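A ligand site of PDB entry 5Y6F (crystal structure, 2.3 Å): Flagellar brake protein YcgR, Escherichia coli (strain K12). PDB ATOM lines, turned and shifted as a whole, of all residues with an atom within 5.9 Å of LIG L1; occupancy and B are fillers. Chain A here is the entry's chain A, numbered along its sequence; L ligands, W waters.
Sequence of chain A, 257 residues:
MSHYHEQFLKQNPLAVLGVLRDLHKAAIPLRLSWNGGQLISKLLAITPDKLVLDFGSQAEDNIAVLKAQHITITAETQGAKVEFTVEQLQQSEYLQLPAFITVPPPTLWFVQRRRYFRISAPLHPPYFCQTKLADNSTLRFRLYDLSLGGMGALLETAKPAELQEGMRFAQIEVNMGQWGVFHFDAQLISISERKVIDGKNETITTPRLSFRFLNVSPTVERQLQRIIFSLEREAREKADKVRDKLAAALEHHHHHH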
ATOM      1  N   ARG A 113     -11.861  26.051   2.813  1.00  0.00           N
ATOM      2  CA  ARG A 113     -11.447  25.607   4.127  1.00  0.00           C
ATOM      3  C   ARG A 113     -10.322  24.592   4.089  1.00  0.00           C
ATOM      4  O   ARG A 113      -9.858  24.168   5.160  1.00  0.00           O
ATOM      5  CB  ARG A 113     -12.637  24.996   4.889  1.00  0.00           C
ATOM      6  CG  ARG A 113     -13.832  25.882   5.016  1.00  0.00           C
ATOM      7  CD  ARG A 113     -15.061  25.061   5.505  1.00  0.00           C
ATOM      8  NE  ARG A 113     -15.757  24.391   4.370  1.00  0.00           N
ATOM      9  CZ  ARG A 113     -16.992  23.920   4.469  1.00  0.00           C
ATOM     10  NH1 ARG A 113     -17.676  24.039   5.611  1.00  0.00           N
ATOM     11  NH2 ARG A 113     -17.561  23.353   3.408  1.00  0.00           N
ATOM     12  N   ARG A 114      -9.912  24.110   2.919  1.00  0.00           N
ATOM     13  CA  ARG A 114      -9.048  22.922   2.851  1.00  0.00           C
ATOM     14  C   ARG A 114      -7.571  23.318   2.948  1.00  0.00           C
ATOM     15  O   ARG A 114      -7.069  24.086   2.128  1.00  0.00           O
ATOM     16  CB  ARG A 114      -9.315  22.137   1.568  1.00  0.00           C
ATOM     17  CG  ARG A 114     -10.796  21.682   1.515  1.00  0.00           C
ATOM     18  CD  ARG A 114     -11.106  21.065   0.169  1.00  0.00           C
ATOM     19  NE  ARG A 114     -12.422  20.483   0.204  1.00  0.00           N
ATOM     20  CZ  ARG A 114     -12.956  19.843  -0.805  1.00  0.00           C
ATOM     21  NH1 ARG A 114     -12.252  19.727  -1.936  1.00  0.00           N
ATOM     22  NH2 ARG A 114     -14.180  19.335  -0.674  1.00  0.00           N
ATOM     23  N   ARG A 115      -6.891  22.794   3.950  1.00  0.00           N
ATOM     24  CA  ARG A 115      -5.459  23.079   4.133  1.00  0.00           C
ATOM     25  C   ARG A 115      -4.617  22.268   3.187  1.00  0.00           C
ATOM     26  O   ARG A 115      -3.518  22.688   2.822  1.00  0.00           O
ATOM     27  CB  ARG A 115      -4.992  22.747   5.542  1.00  0.00           C
ATOM     28  CG  ARG A 115      -5.832  23.384   6.657  1.00  0.00           C
ATOM     29  CD  ARG A 115      -5.725  22.622   8.000  1.00  0.00           C
ATOM     30  NE  ARG A 115      -6.454  21.359   7.900  1.00  0.00           N
ATOM     31  CZ  ARG A 115      -6.608  20.491   8.888  1.00  0.00           C
ATOM     32  NH1 ARG A 115      -6.099  20.760  10.093  1.00  0.00           N
ATOM     33  NH2 ARG A 115      -7.247  19.348   8.675  1.00  0.00           N
ATOM     34  N   TYR A 116      -5.125  21.098   2.771  1.00  0.00           N
ATOM     35  CA  TYR A 116      -4.295  20.143   2.050  1.00  0.00           C
ATOM     36  C   TYR A 116      -4.860  19.923   0.673  1.00  0.00           C
ATOM     37  O   TYR A 116      -6.071  20.032   0.435  1.00  0.00           O
ATOM     38  CB  TYR A 116      -4.192  18.795   2.803  1.00  0.00           C
ATOM     39  CG  TYR A 116      -3.831  18.905   4.284  1.00  0.00           C
ATOM     40  CD1 TYR A 116      -2.635  19.490   4.679  1.00  0.00           C
ATOM     41  CD2 TYR A 116      -4.695  18.391   5.262  1.00  0.00           C
ATOM     42  CE1 TYR A 116      -2.297  19.589   6.012  1.00  0.00           C
ATOM     43  CE2 TYR A 116      -4.389  18.508   6.602  1.00  0.00           C
ATOM     44  CZ  TYR A 116      -3.175  19.114   6.972  1.00  0.00           C
ATOM     45  OH  TYR A 116      -2.826  19.241   8.299  1.00  0.00           O
ATOM     46  N   ARG A 118      -5.983  17.780  -2.497  1.00  0.00           N
ATOM     47  CA  ARG A 118      -6.665  16.504  -2.694  1.00  0.00           C
ATOM     48  C   ARG A 118      -6.443  16.028  -4.113  1.00  0.00           C
ATOM     49  O   ARG A 118      -6.673  16.770  -5.070  1.00  0.00           O
ATOM     50  CB  ARG A 118      -8.151  16.649  -2.420  1.00  0.00           C
ATOM     51  CG  ARG A 118      -8.454  17.194  -1.033  1.00  0.00           C
ATOM     52  CD  ARG A 118      -9.935  17.024  -0.679  1.00  0.00           C
ATOM     53  NE  ARG A 118     -10.199  17.545   0.680  1.00  0.00           N
ATOM     54  CZ  ARG A 118     -11.361  17.408   1.330  1.00  0.00           C
ATOM     55  NH1 ARG A 118     -12.413  16.764   0.741  1.00  0.00           N
ATOM     56  NH2 ARG A 118     -11.467  17.877   2.578  1.00  0.00           N
ATOM     57  N   ILE A 119      -6.014  14.796  -4.255  1.00  0.00           N
ATOM     58  CA  ILE A 119      -5.820  14.212  -5.563  1.00  0.00           C
ATOM     59  C   ILE A 119      -6.835  13.087  -5.731  1.00  0.00           C
ATOM     60  O   ILE A 119      -7.139  12.366  -4.777  1.00  0.00           O
ATOM     61  CB  ILE A 119      -4.378  13.715  -5.754  1.00  0.00           C
ATOM     62  CG1 ILE A 119      -4.155  13.328  -7.217  1.00  0.00           C
ATOM     63  CG2 ILE A 119      -4.030  12.563  -4.831  1.00  0.00           C
ATOM     64  CD1 ILE A 119      -2.782  13.726  -7.677  1.00  0.00           C
ATOM     65  N   ASP A 145     -10.732   9.981  -3.405  1.00  0.00           N
ATOM     66  CA  ASP A 145      -9.648  10.943  -3.436  1.00  0.00           C
ATOM     67  C   ASP A 145      -8.860  10.857  -2.131  1.00  0.00           C
ATOM     68  O   ASP A 145      -9.257  10.148  -1.189  1.00  0.00           O
ATOM     69  CB  ASP A 145     -10.160  12.360  -3.755  1.00  0.00           C
ATOM     70  CG  ASP A 145     -10.999  12.961  -2.618  1.00  0.00           C
ATOM     71  OD1 ASP A 145     -10.985  12.463  -1.472  1.00  0.00           O
ATOM     72  OD2 ASP A 145     -11.679  13.974  -2.899  1.00  0.00           O
ATOM     73  N   LEU A 146      -7.749  11.583  -2.087  1.00  0.00           N
ATOM     74  CA  LEU A 146      -6.747  11.391  -1.053  1.00  0.00           C
ATOM     75  C   LEU A 146      -6.083  12.722  -0.781  1.00  0.00           C
ATOM     76  O   LEU A 146      -5.753  13.449  -1.708  1.00  0.00           O
ATOM     77  CB  LEU A 146      -5.680  10.384  -1.493  1.00  0.00           C
ATOM     78  CG  LEU A 146      -4.635  10.049  -0.455  1.00  0.00           C
ATOM     79  CD1 LEU A 146      -5.339   9.417   0.725  1.00  0.00           C
ATOM     80  CD2 LEU A 146      -3.575   9.110  -1.021  1.00  0.00           C
ATOM     81  N   SER A 147      -5.896  13.005   0.495  1.00  0.00           N
ATOM     82  CA  SER A 147      -5.200  14.190   0.943  1.00  0.00           C
ATOM     83  C   SER A 147      -4.359  13.767   2.143  1.00  0.00           C
ATOM     84  O   SER A 147      -4.516  12.668   2.664  1.00  0.00           O
ATOM     85  CB  SER A 147      -6.152  15.312   1.325  1.00  0.00           C
ATOM     86  OG  SER A 147      -6.632  15.175   2.651  1.00  0.00           O
ATOM     87  N   LEU A 148      -3.501  14.668   2.600  1.00  0.00           N
ATOM     88  CA  LEU A 148      -2.678  14.372   3.765  1.00  0.00           C
ATOM     89  C   LEU A 148      -3.502  14.068   5.016  1.00  0.00           C
ATOM     90  O   LEU A 148      -3.019  13.391   5.900  1.00  0.00           O
ATOM     91  CB  LEU A 148      -1.759  15.560   4.042  1.00  0.00           C
ATOM     92  CG  LEU A 148      -0.439  15.338   4.731  1.00  0.00           C
ATOM     93  CD1 LEU A 148       0.352  14.411   3.857  1.00  0.00           C
ATOM     94  CD2 LEU A 148       0.246  16.685   4.856  1.00  0.00           C
ATOM     95  N   GLY A 149      -4.725  14.566   5.115  1.00  0.00           N
ATOM     96  CA  GLY A 149      -5.463  14.398   6.345  1.00  0.00           C
ATOM     97  C   GLY A 149      -6.634  13.455   6.263  1.00  0.00           C
ATOM     98  O   GLY A 149      -7.359  13.284   7.265  1.00  0.00           O
ATOM     99  N   GLY A 150      -6.830  12.795   5.122  1.00  0.00           N
ATOM    100  CA  GLY A 150      -8.013  11.973   4.986  1.00  0.00           C
ATOM    101  C   GLY A 150      -8.235  11.511   3.569  1.00  0.00           C
ATOM    102  O   GLY A 150      -7.328  11.555   2.731  1.00  0.00           O
ATOM    103  N   MET A 151      -9.454  11.057   3.325  1.00  0.00           N
ATOM    104  CA  MET A 151      -9.704  10.326   2.109  1.00  0.00           C
ATOM    105  C   MET A 151     -11.202  10.319   1.894  1.00  0.00           C
ATOM    106  O   MET A 151     -11.981  10.330   2.859  1.00  0.00           O
ATOM    107  CB  MET A 151      -9.139   8.886   2.216  1.00  0.00           C
ATOM    108  CG  MET A 151      -9.819   8.064   3.325  1.00  0.00           C
ATOM    109  SD  MET A 151      -9.479   6.269   3.362  1.00  0.00           S
ATOM    110  CE  MET A 151      -8.093   6.150   2.235  1.00  0.00           C
ATOM    111  N   GLY A 152     -11.601  10.318   0.641  1.00  0.00           N
ATOM    112  CA  GLY A 152     -12.971  10.131   0.253  1.00  0.00           C
ATOM    113  C   GLY A 152     -13.107   8.748  -0.357  1.00  0.00           C
ATOM    114  O   GLY A 152     -12.157   8.237  -0.968  1.00  0.00           O
ATOM    115  N   ALA A 153     -14.268   8.132  -0.182  1.00  0.00           N
ATOM    116  CA  ALA A 153     -14.487   6.755  -0.615  1.00  0.00           C
ATOM    117  C   ALA A 153     -15.877   6.647  -1.196  1.00  0.00           C
ATOM    118  O   ALA A 153     -16.787   7.365  -0.762  1.00  0.00           O
ATOM    119  CB  ALA A 153     -14.351   5.745   0.544  1.00  0.00           C
ATOM    120  N   ILE A 189     -16.638  11.041   8.881  1.00  0.00           N
ATOM    121  CA  ILE A 189     -17.098  12.368   9.239  1.00  0.00           C
ATOM    122  C   ILE A 189     -18.278  12.837   8.401  1.00  0.00           C
ATOM    123  O   ILE A 189     -18.996  13.748   8.829  1.00  0.00           O
ATOM    124  CB  ILE A 189     -15.962  13.410   9.159  1.00  0.00           C
ATOM    125  CG1 ILE A 189     -15.457  13.515   7.723  1.00  0.00           C
ATOM    126  CG2 ILE A 189     -14.855  13.081  10.152  1.00  0.00           C
ATOM    127  CD1 ILE A 189     -14.238  14.377   7.585  1.00  0.00           C
ATOM    128  N   SER A 190     -18.492  12.251   7.234  1.00  0.00           N
ATOM    129  CA  SER A 190     -19.625  12.699   6.435  1.00  0.00           C
ATOM    130  C   SER A 190     -20.101  11.563   5.555  1.00  0.00           C
ATOM    131  O   SER A 190     -19.277  10.817   4.995  1.00  0.00           O
ATOM    132  CB  SER A 190     -19.285  13.934   5.574  1.00  0.00           C
ATOM    133  OG  SER A 190     -20.489  14.477   5.077  1.00  0.00           O
ATOM    134  N   ARG A 208     -21.262   8.217  -0.887  1.00  0.00           N
ATOM    135  CA  ARG A 208     -19.912   8.723  -0.689  1.00  0.00           C
ATOM    136  C   ARG A 208     -19.604   8.920   0.794  1.00  0.00           C
ATOM    137  O   ARG A 208     -20.413   9.506   1.534  1.00  0.00           O
ATOM    138  CB  ARG A 208     -19.765  10.041  -1.447  1.00  0.00           C
ATOM    139  CG  ARG A 208     -18.756  11.011  -0.895  1.00  0.00           C
ATOM    140  CD  ARG A 208     -17.532  11.012  -1.761  1.00  0.00           C
ATOM    141  NE  ARG A 208     -16.446  11.682  -1.064  1.00  0.00           N
ATOM    142  CZ  ARG A 208     -15.927  12.820  -1.476  1.00  0.00           C
ATOM    143  NH1 ARG A 208     -16.374  13.389  -2.575  1.00  0.00           N
ATOM    144  NH2 ARG A 208     -14.934  13.361  -0.803  1.00  0.00           N
ATOM    145  N   LEU A 209     -18.427   8.443   1.220  1.00  0.00           N
ATOM    146  CA  LEU A 209     -17.922   8.604   2.585  1.00  0.00           C
ATOM    147  C   LEU A 209     -16.740   9.570   2.617  1.00  0.00           C
ATOM    148  O   LEU A 209     -15.948   9.644   1.668  1.00  0.00           O
ATOM    149  CB  LEU A 209     -17.460   7.273   3.181  1.00  0.00           C
ATOM    150  CG  LEU A 209     -18.502   6.163   3.397  1.00  0.00           C
ATOM    151  CD1 LEU A 209     -19.167   5.837   2.095  1.00  0.00           C
ATOM    152  CD2 LEU A 209     -17.848   4.907   3.981  1.00  0.00           C
ATOM    153  N   SER A 210     -16.615  10.274   3.728  1.00  0.00           N
ATOM    154  CA  SER A 210     -15.519  11.199   3.953  1.00  0.00           C
ATOM    155  C   SER A 210     -14.857  10.819   5.274  1.00  0.00           C
ATOM    156  O   SER A 210     -15.538  10.716   6.298  1.00  0.00           O
ATOM    157  CB  SER A 210     -16.033  12.632   4.002  1.00  0.00           C
ATOM    158  OG  SER A 210     -16.196  13.250   2.708  1.00  0.00           O
ATOM    159  N   PHE A 211     -13.545  10.561   5.239  1.00  0.00           N
ATOM    160  CA  PHE A 211     -12.788  10.120   6.400  1.00  0.00           C
ATOM    161  C   PHE A 211     -11.719  11.142   6.697  1.00  0.00           C
ATOM    162  O   PHE A 211     -11.007  11.566   5.790  1.00  0.00           O
ATOM    163  CB  PHE A 211     -12.129   8.763   6.178  1.00  0.00           C
ATOM    164  CG  PHE A 211     -13.077   7.609   6.248  1.00  0.00           C
ATOM    165  CD1 PHE A 211     -13.424   7.054   7.479  1.00  0.00           C
ATOM    166  CD2 PHE A 211     -13.641   7.072   5.094  1.00  0.00           C
ATOM    167  CE1 PHE A 211     -14.297   6.003   7.555  1.00  0.00           C
ATOM    168  CE2 PHE A 211     -14.532   5.996   5.153  1.00  0.00           C
ATOM    169  CZ  PHE A 211     -14.852   5.454   6.389  1.00  0.00           C
ATOM    170  N   ARG A 212     -11.608  11.523   7.963  1.00  0.00           N
ATOM    171  CA  ARG A 212     -10.420  12.213   8.435  1.00  0.00           C
ATOM    172  C   ARG A 212      -9.568  11.209   9.178  1.00  0.00           C
ATOM    173  O   ARG A 212     -10.098  10.435   9.984  1.00  0.00           O
ATOM    174  CB  ARG A 212     -10.784  13.386   9.342  1.00  0.00           C
ATOM    175  CG  ARG A 212     -11.433  13.023  10.695  1.00  0.00           C
ATOM    176  CD  ARG A 212     -11.515  14.313  11.543  1.00  0.00           C
ATOM    177  NE  ARG A 212     -12.326  14.155  12.729  1.00  0.00           N
ATOM    178  CZ  ARG A 212     -13.318  14.968  13.073  1.00  0.00           C
ATOM    179  NH1 ARG A 212     -13.616  16.035  12.320  1.00  0.00           N
ATOM    180  NH2 ARG A 212     -14.010  14.730  14.183  1.00  0.00           N
ATOM    181  N   PHE A 213      -8.254  11.198   8.901  1.00  0.00           N
ATOM    182  CA  PHE A 213      -7.346  10.267   9.589  1.00  0.00           C
ATOM    183  C   PHE A 213      -7.085  10.709  11.022  1.00  0.00           C
ATOM    184  O   PHE A 213      -6.891  11.888  11.308  1.00  0.00           O
ATOM    185  CB  PHE A 213      -5.985  10.162   8.897  1.00  0.00           C
ATOM    186  CG  PHE A 213      -6.044   9.657   7.493  1.00  0.00           C
ATOM    187  CD1 PHE A 213      -6.907   8.655   7.123  1.00  0.00           C
ATOM    188  CD2 PHE A 213      -5.187  10.178   6.534  1.00  0.00           C
ATOM    189  CE1 PHE A 213      -6.913   8.191   5.808  1.00  0.00           C
ATOM    190  CE2 PHE A 213      -5.196   9.714   5.234  1.00  0.00           C
ATOM    191  CZ  PHE A 213      -6.059   8.729   4.878  1.00  0.00           C
HETATM  192  P1  LIG L   1      -9.126  19.973   5.249  1.00  0.00           P
HETATM  193  O1  LIG L   1      -9.142  19.528   3.716  1.00  0.00           O
HETATM  194  O2  LIG L   1      -8.015  20.900   5.499  1.00  0.00           O
HETATM  195  O3  LIG L   1     -10.560  20.570   5.614  1.00  0.00           O
HETATM  196  C1  LIG L   1     -10.582  21.306   6.831  1.00  0.00           C
HETATM  197  C2  LIG L   1     -11.986  21.405   7.420  1.00  0.00           C
HETATM  198  O4  LIG L   1     -12.846  22.136   6.557  1.00  0.00           O
HETATM  199  C3  LIG L   1     -12.654  20.024   7.566  1.00  0.00           C
HETATM  200  O5  LIG L   1     -12.403  19.442   8.835  1.00  0.00           O
HETATM  201  C4  LIG L   1     -14.135  20.353   7.442  1.00  0.00           C
HETATM  202  O6  LIG L   1     -14.558  20.943   8.651  1.00  0.00           O
HETATM  203  C5  LIG L   1     -14.121  21.497   6.406  1.00  0.00           C
HETATM  204  N1  LIG L   1     -14.317  21.059   5.030  1.00  0.00           N
HETATM  205  C6  LIG L   1     -13.340  20.951   4.079  1.00  0.00           C
HETATM  206  N2  LIG L   1     -13.874  20.555   2.957  1.00  0.00           N
HETATM  207  C7  LIG L   1     -15.225  20.369   3.143  1.00  0.00           C
HETATM  208  C8  LIG L   1     -16.308  19.960   2.334  1.00  0.00           C
HETATM  209  O7  LIG L   1     -16.233  19.654   1.149  1.00  0.00           O
HETATM  210  N3  LIG L   1     -17.519  19.916   2.900  1.00  0.00           N
HETATM  211  C9  LIG L   1     -17.693  20.221   4.195  1.00  0.00           C
HETATM  212  N4  LIG L   1     -18.955  20.106   4.673  1.00  0.00           N
HETATM  213  N5  LIG L   1     -16.720  20.593   4.967  1.00  0.00           N
HETATM  214  C10 LIG L   1     -15.495  20.698   4.475  1.00  0.00           C
HETATM  215  P2  LIG L   1     -12.651  17.844   9.064  1.00  0.00           P
HETATM  216  O8  LIG L   1     -14.091  17.535   8.469  1.00  0.00           O
HETATM  217  O9  LIG L   1     -12.443  17.573  10.506  1.00  0.00           O
HETATM  218  O10 LIG L   1     -11.607  17.023   8.139  1.00  0.00           O
HETATM  219  C11 LIG L   1     -10.222  17.114   8.446  1.00  0.00           C
HETATM  220  C12 LIG L   1      -9.441  16.590   7.252  1.00  0.00           C
HETATM  221  O11 LIG L   1     -10.002  15.356   6.804  1.00  0.00           O
HETATM  222  C13 LIG L   1      -9.610  17.491   6.009  1.00  0.00           C
HETATM  223  O12 LIG L   1      -8.849  18.682   6.175  1.00  0.00           O
HETATM  224  C14 LIG L   1      -9.055  16.591   4.913  1.00  0.00           C
HETATM  225  O13 LIG L   1      -7.649  16.685   4.942  1.00  0.00           O
HETATM  226  C15 LIG L   1      -9.531  15.206   5.453  1.00  0.00           C
HETATM  227  N6  LIG L   1     -10.706  14.807   4.747  1.00  0.00           N
HETATM  228  C16 LIG L   1     -11.985  14.842   5.248  1.00  0.00           C
HETATM  229  N7  LIG L   1     -12.829  14.425   4.322  1.00  0.00           N
HETATM  230  C17 LIG L   1     -12.081  14.076   3.226  1.00  0.00           C
HETATM  231  C18 LIG L   1     -12.430  13.617   1.993  1.00  0.00           C
HETATM  232  O14 LIG L   1     -13.601  13.396   1.696  1.00  0.00           O
HETATM  233  N8  LIG L   1     -11.441  13.446   1.131  1.00  0.00           N
HETATM  234  C19 LIG L   1     -10.166  13.700   1.448  1.00  0.00           C
HETATM  235  N9  LIG L   1      -9.192  13.474   0.505  1.00  0.00           N
HETATM  236  N10 LIG L   1      -9.816  14.142   2.603  1.00  0.00           N
HETATM  237  C20 LIG L   1     -10.756  14.345   3.481  1.00  0.00           C
HETATM  238  P1  LG2 L   2     -16.724  17.097  -2.612  1.00  0.00           P
HETATM  239  O1  LG2 L   2     -15.184  17.522  -2.503  1.00  0.00           O
HETATM  240  O2  LG2 L   2     -16.887  15.980  -3.586  1.00  0.00           O
HETATM  241  O3  LG2 L   2     -17.287  16.703  -1.169  1.00  0.00           O
HETATM  242  C1  LG2 L   2     -18.598  16.050  -1.168  1.00  0.00           C
HETATM  243  C2  LG2 L   2     -19.144  15.883   0.224  1.00  0.00           C
HETATM  244  O4  LG2 L   2     -18.217  15.141   0.999  1.00  0.00           O
HETATM  245  C3  LG2 L   2     -19.233  17.238   0.904  1.00  0.00           C
HETATM  246  O5  LG2 L   2     -20.464  17.875   0.609  1.00  0.00           O
HETATM  247  C4  LG2 L   2     -19.214  16.814   2.359  1.00  0.00           C
HETATM  248  O6  LG2 L   2     -20.439  16.252   2.788  1.00  0.00           O
HETATM  249  C5  LG2 L   2     -18.201  15.685   2.300  1.00  0.00           C
HETATM  250  N1  LG2 L   2     -16.854  16.197   2.555  1.00  0.00           N
HETATM  251  C6  LG2 L   2     -15.827  16.336   1.682  1.00  0.00           C
HETATM  252  N2  LG2 L   2     -14.780  16.773   2.324  1.00  0.00           N
HETATM  253  C7  LG2 L   2     -15.101  16.936   3.620  1.00  0.00           C
HETATM  254  C8  LG2 L   2     -14.399  17.382   4.739  1.00  0.00           C
HETATM  255  O7  LG2 L   2     -13.228  17.717   4.658  1.00  0.00           O
HETATM  256  N3  LG2 L   2     -15.040  17.397   5.906  1.00  0.00           N
HETATM  257  C9  LG2 L   2     -16.348  17.018   5.989  1.00  0.00           C
HETATM  258  N4  LG2 L   2     -16.997  17.081   7.197  1.00  0.00           N
HETATM  259  N5  LG2 L   2     -17.009  16.621   4.942  1.00  0.00           N
HETATM  260  C10 LG2 L   2     -16.422  16.558   3.772  1.00  0.00           C
HETATM  261  P2  LG2 L   2     -20.692  19.432   0.787  1.00  0.00           P
HETATM  262  O8  LG2 L   2     -20.117  19.985   2.188  1.00  0.00           O
HETATM  263  O9  LG2 L   2     -22.052  19.819   0.426  1.00  0.00           O
HETATM  264  O10 LG2 L   2     -19.756  20.054  -0.353  1.00  0.00           O
HETATM  265  C11 LG2 L   2     -20.129  19.861  -1.690  1.00  0.00           C
HETATM  266  C12 LG2 L   2     -18.992  20.257  -2.646  1.00  0.00           C
HETATM  267  O11 LG2 L   2     -18.601  21.619  -2.481  1.00  0.00           O
HETATM  268  C13 LG2 L   2     -17.738  19.468  -2.337  1.00  0.00           C
HETATM  269  O12 LG2 L   2     -17.713  18.256  -3.083  1.00  0.00           O
HETATM  270  C14 LG2 L   2     -16.641  20.404  -2.878  1.00  0.00           C
HETATM  271  O13 LG2 L   2     -16.697  20.551  -4.293  1.00  0.00           O
HETATM  272  C15 LG2 L   2     -17.174  21.750  -2.477  1.00  0.00           C
HETATM  273  N6  LG2 L   2     -16.647  22.297  -1.215  1.00  0.00           N
HETATM  274  C16 LG2 L   2     -17.271  22.462  -0.033  1.00  0.00           C
HETATM  275  N7  LG2 L   2     -16.499  23.054   0.788  1.00  0.00           N
HETATM  276  C17 LG2 L   2     -15.306  23.296   0.192  1.00  0.00           C
HETATM  277  C18 LG2 L   2     -14.120  23.917   0.607  1.00  0.00           C
HETATM  278  O14 LG2 L   2     -14.074  24.348   1.743  1.00  0.00           O
HETATM  279  N8  LG2 L   2     -13.078  23.977  -0.269  1.00  0.00           N
HETATM  280  C19 LG2 L   2     -13.227  23.493  -1.548  1.00  0.00           C
HETATM  281  N9  LG2 L   2     -12.174  23.627  -2.430  1.00  0.00           N
HETATM  282  N10 LG2 L   2     -14.380  22.948  -1.971  1.00  0.00           N
HETATM  283  C20 LG2 L   2     -15.388  22.823  -1.116  1.00  0.00           C
HETATM  284  O   HOH W   1     -10.017  24.656   7.589  1.00  0.00           O
HETATM  285  O   HOH W   2     -20.265  22.490   2.691  1.00  0.00           O
HETATM  286  O   HOH W   3      -7.852  18.293   2.062  1.00  0.00           O
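An oxygen (O9) of LIG L1 is in salt-bridge range of the guanidinium group (NH1) of Arg 212, at 2.7 Å. The backbone NH (N) of Arg 115 lies within hydrogen-bond range of an oxygen (O2) of LIG L1, at 2.7 Å. NE of Arg 115 is in salt-bridge range of O2 of LIG L1 (2.9 Å). The guanidinium group (NH2) of Arg 114 sits at hydrogen-bond distance from an oxygen (O7) of LIG L1, at 2.8 Å. OG of Ser 210 is in hydrogen-bond range of O14 of LIG L1. The side-chain carboxylate (OD1) of Asp 145 is in hydrogen-bond range of a nitrogen (N8) of LIG L1 (2.8 Å). The guanidinium group (NH2) of Arg 208 is in hydrogen-bond range of an oxygen (O14) of LIG L1, at 2.8 Å. OG of Ser 147 lies within hydrogen-bond range of O13 of LIG L1, at 2.9 Å. The guanidinium group (NH2) of Arg 118 is in salt-bridge range of an oxygen (O1) of LIG L1 (3.1 Å). N of Met 151 sits at hydrogen-bond distance from N10 of LIG L1, at 3.2 Å. The backbone carbonyl oxygen (O) of Gly 150 sits at hydrogen-bond distance from a nitrogen (N9) of LIG L1, at 3.5 Å. NH2 of Arg 113 sits close to N5 of LIG L1 (3.3 Å). An oxygen (O1) of LG2 L2 lies within salt-bridge range of the guanidinium group of Arg 114 (2.8 Å). The side-chain hydroxyl of Ser 210 sits close to an oxygen (O4) of LG2 L2, 3.3 Å away. The guanidinium group of Arg 208 lies within salt-bridge range of an oxygen (O2) of LG2 L2 (2.8 Å). O7 of LG2 L2 is in hydrogen-bond range of NH2 of Arg 118. N of Arg 113 lies within hydrogen-bond range of O14 of LG2 L2, 3.0 Å away. A nitrogen (N7) of LG2 L2 lies within hydrogen-bond range of the guanidinium group (NH2) of Arg 113 (2.8 Å). O6 of LG2 L2 is in hydrogen-bond range of OG of Ser 190 (2.9 Å).
N3 of LIG L1 lies within hydrogen-bond range of O8 of LG2 L2, 2.7 Å away.
The backbone NH (N) of Ile 189 sits at hydrogen-bond distance from the backbone carbonyl oxygen (O) of Ser 210 (2.8 Å). N of Ser 210 sits at hydrogen-bond distance from O of Ser 190, 3.0 Å away. OD2 of Asp 145 is in salt-bridge range of NH2 of Arg 208 (3.9 Å). O of Asp 145 lies within hydrogen-bond range of N of Gly 152. The side-chain hydroxyl (OG) of Ser 147 sits at hydrogen-bond distance from the backbone NH (N) of Gly 150 (3.4 Å). OG of Ser 147 sits close to N of Gly 149 (3.2 Å). The backbone carbonyl oxygen (O) of Met 151 lies within hydrogen-bond range of the backbone NH (N) of Phe 211, 2.9 Å away. The backbone carbonyl oxygen (O) of Ile 119 lies within hydrogen-bond range of the backbone NH (N) of Leu 146, at 2.9 Å.
O of Gly 149 sits close to O11 of LIG L1, at 3.4 Å. N of Gly 152 lies close to N8 of LIG L1, at 3.2 Å. A nitrogen (N6) of LIG L1 lies close to the backbone carbonyl oxygen of Phe 211 (3.4 Å). Tyr 116 touches LIG L1 (CD2 to O13, 3.4 Å). Leu 146 touches LIG L1. Ile 189 touches LIG L1 (CD1 to C16, 3.3 Å). Hydrophobic or aromatic side chains that line LIG L1: Tyr 116 and Ile 189. The nearest printed residue that does not touch LIG L1 is Leu 209 (4.4 Å).
Water W3 lies within hydrogen-bond range of an oxygen (O1) of LIG L1, the guanidinium group of Arg 118, the backbone carbonyl oxygen of Tyr 116 and the side-chain hydroxyl of Ser 147. Water W2 lies within hydrogen-bond range of O8 of LG2 L2 (2.6 Å), NH2 of Arg 113 (2.9 Å) and N4 of LIG L1 (3.4 Å).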
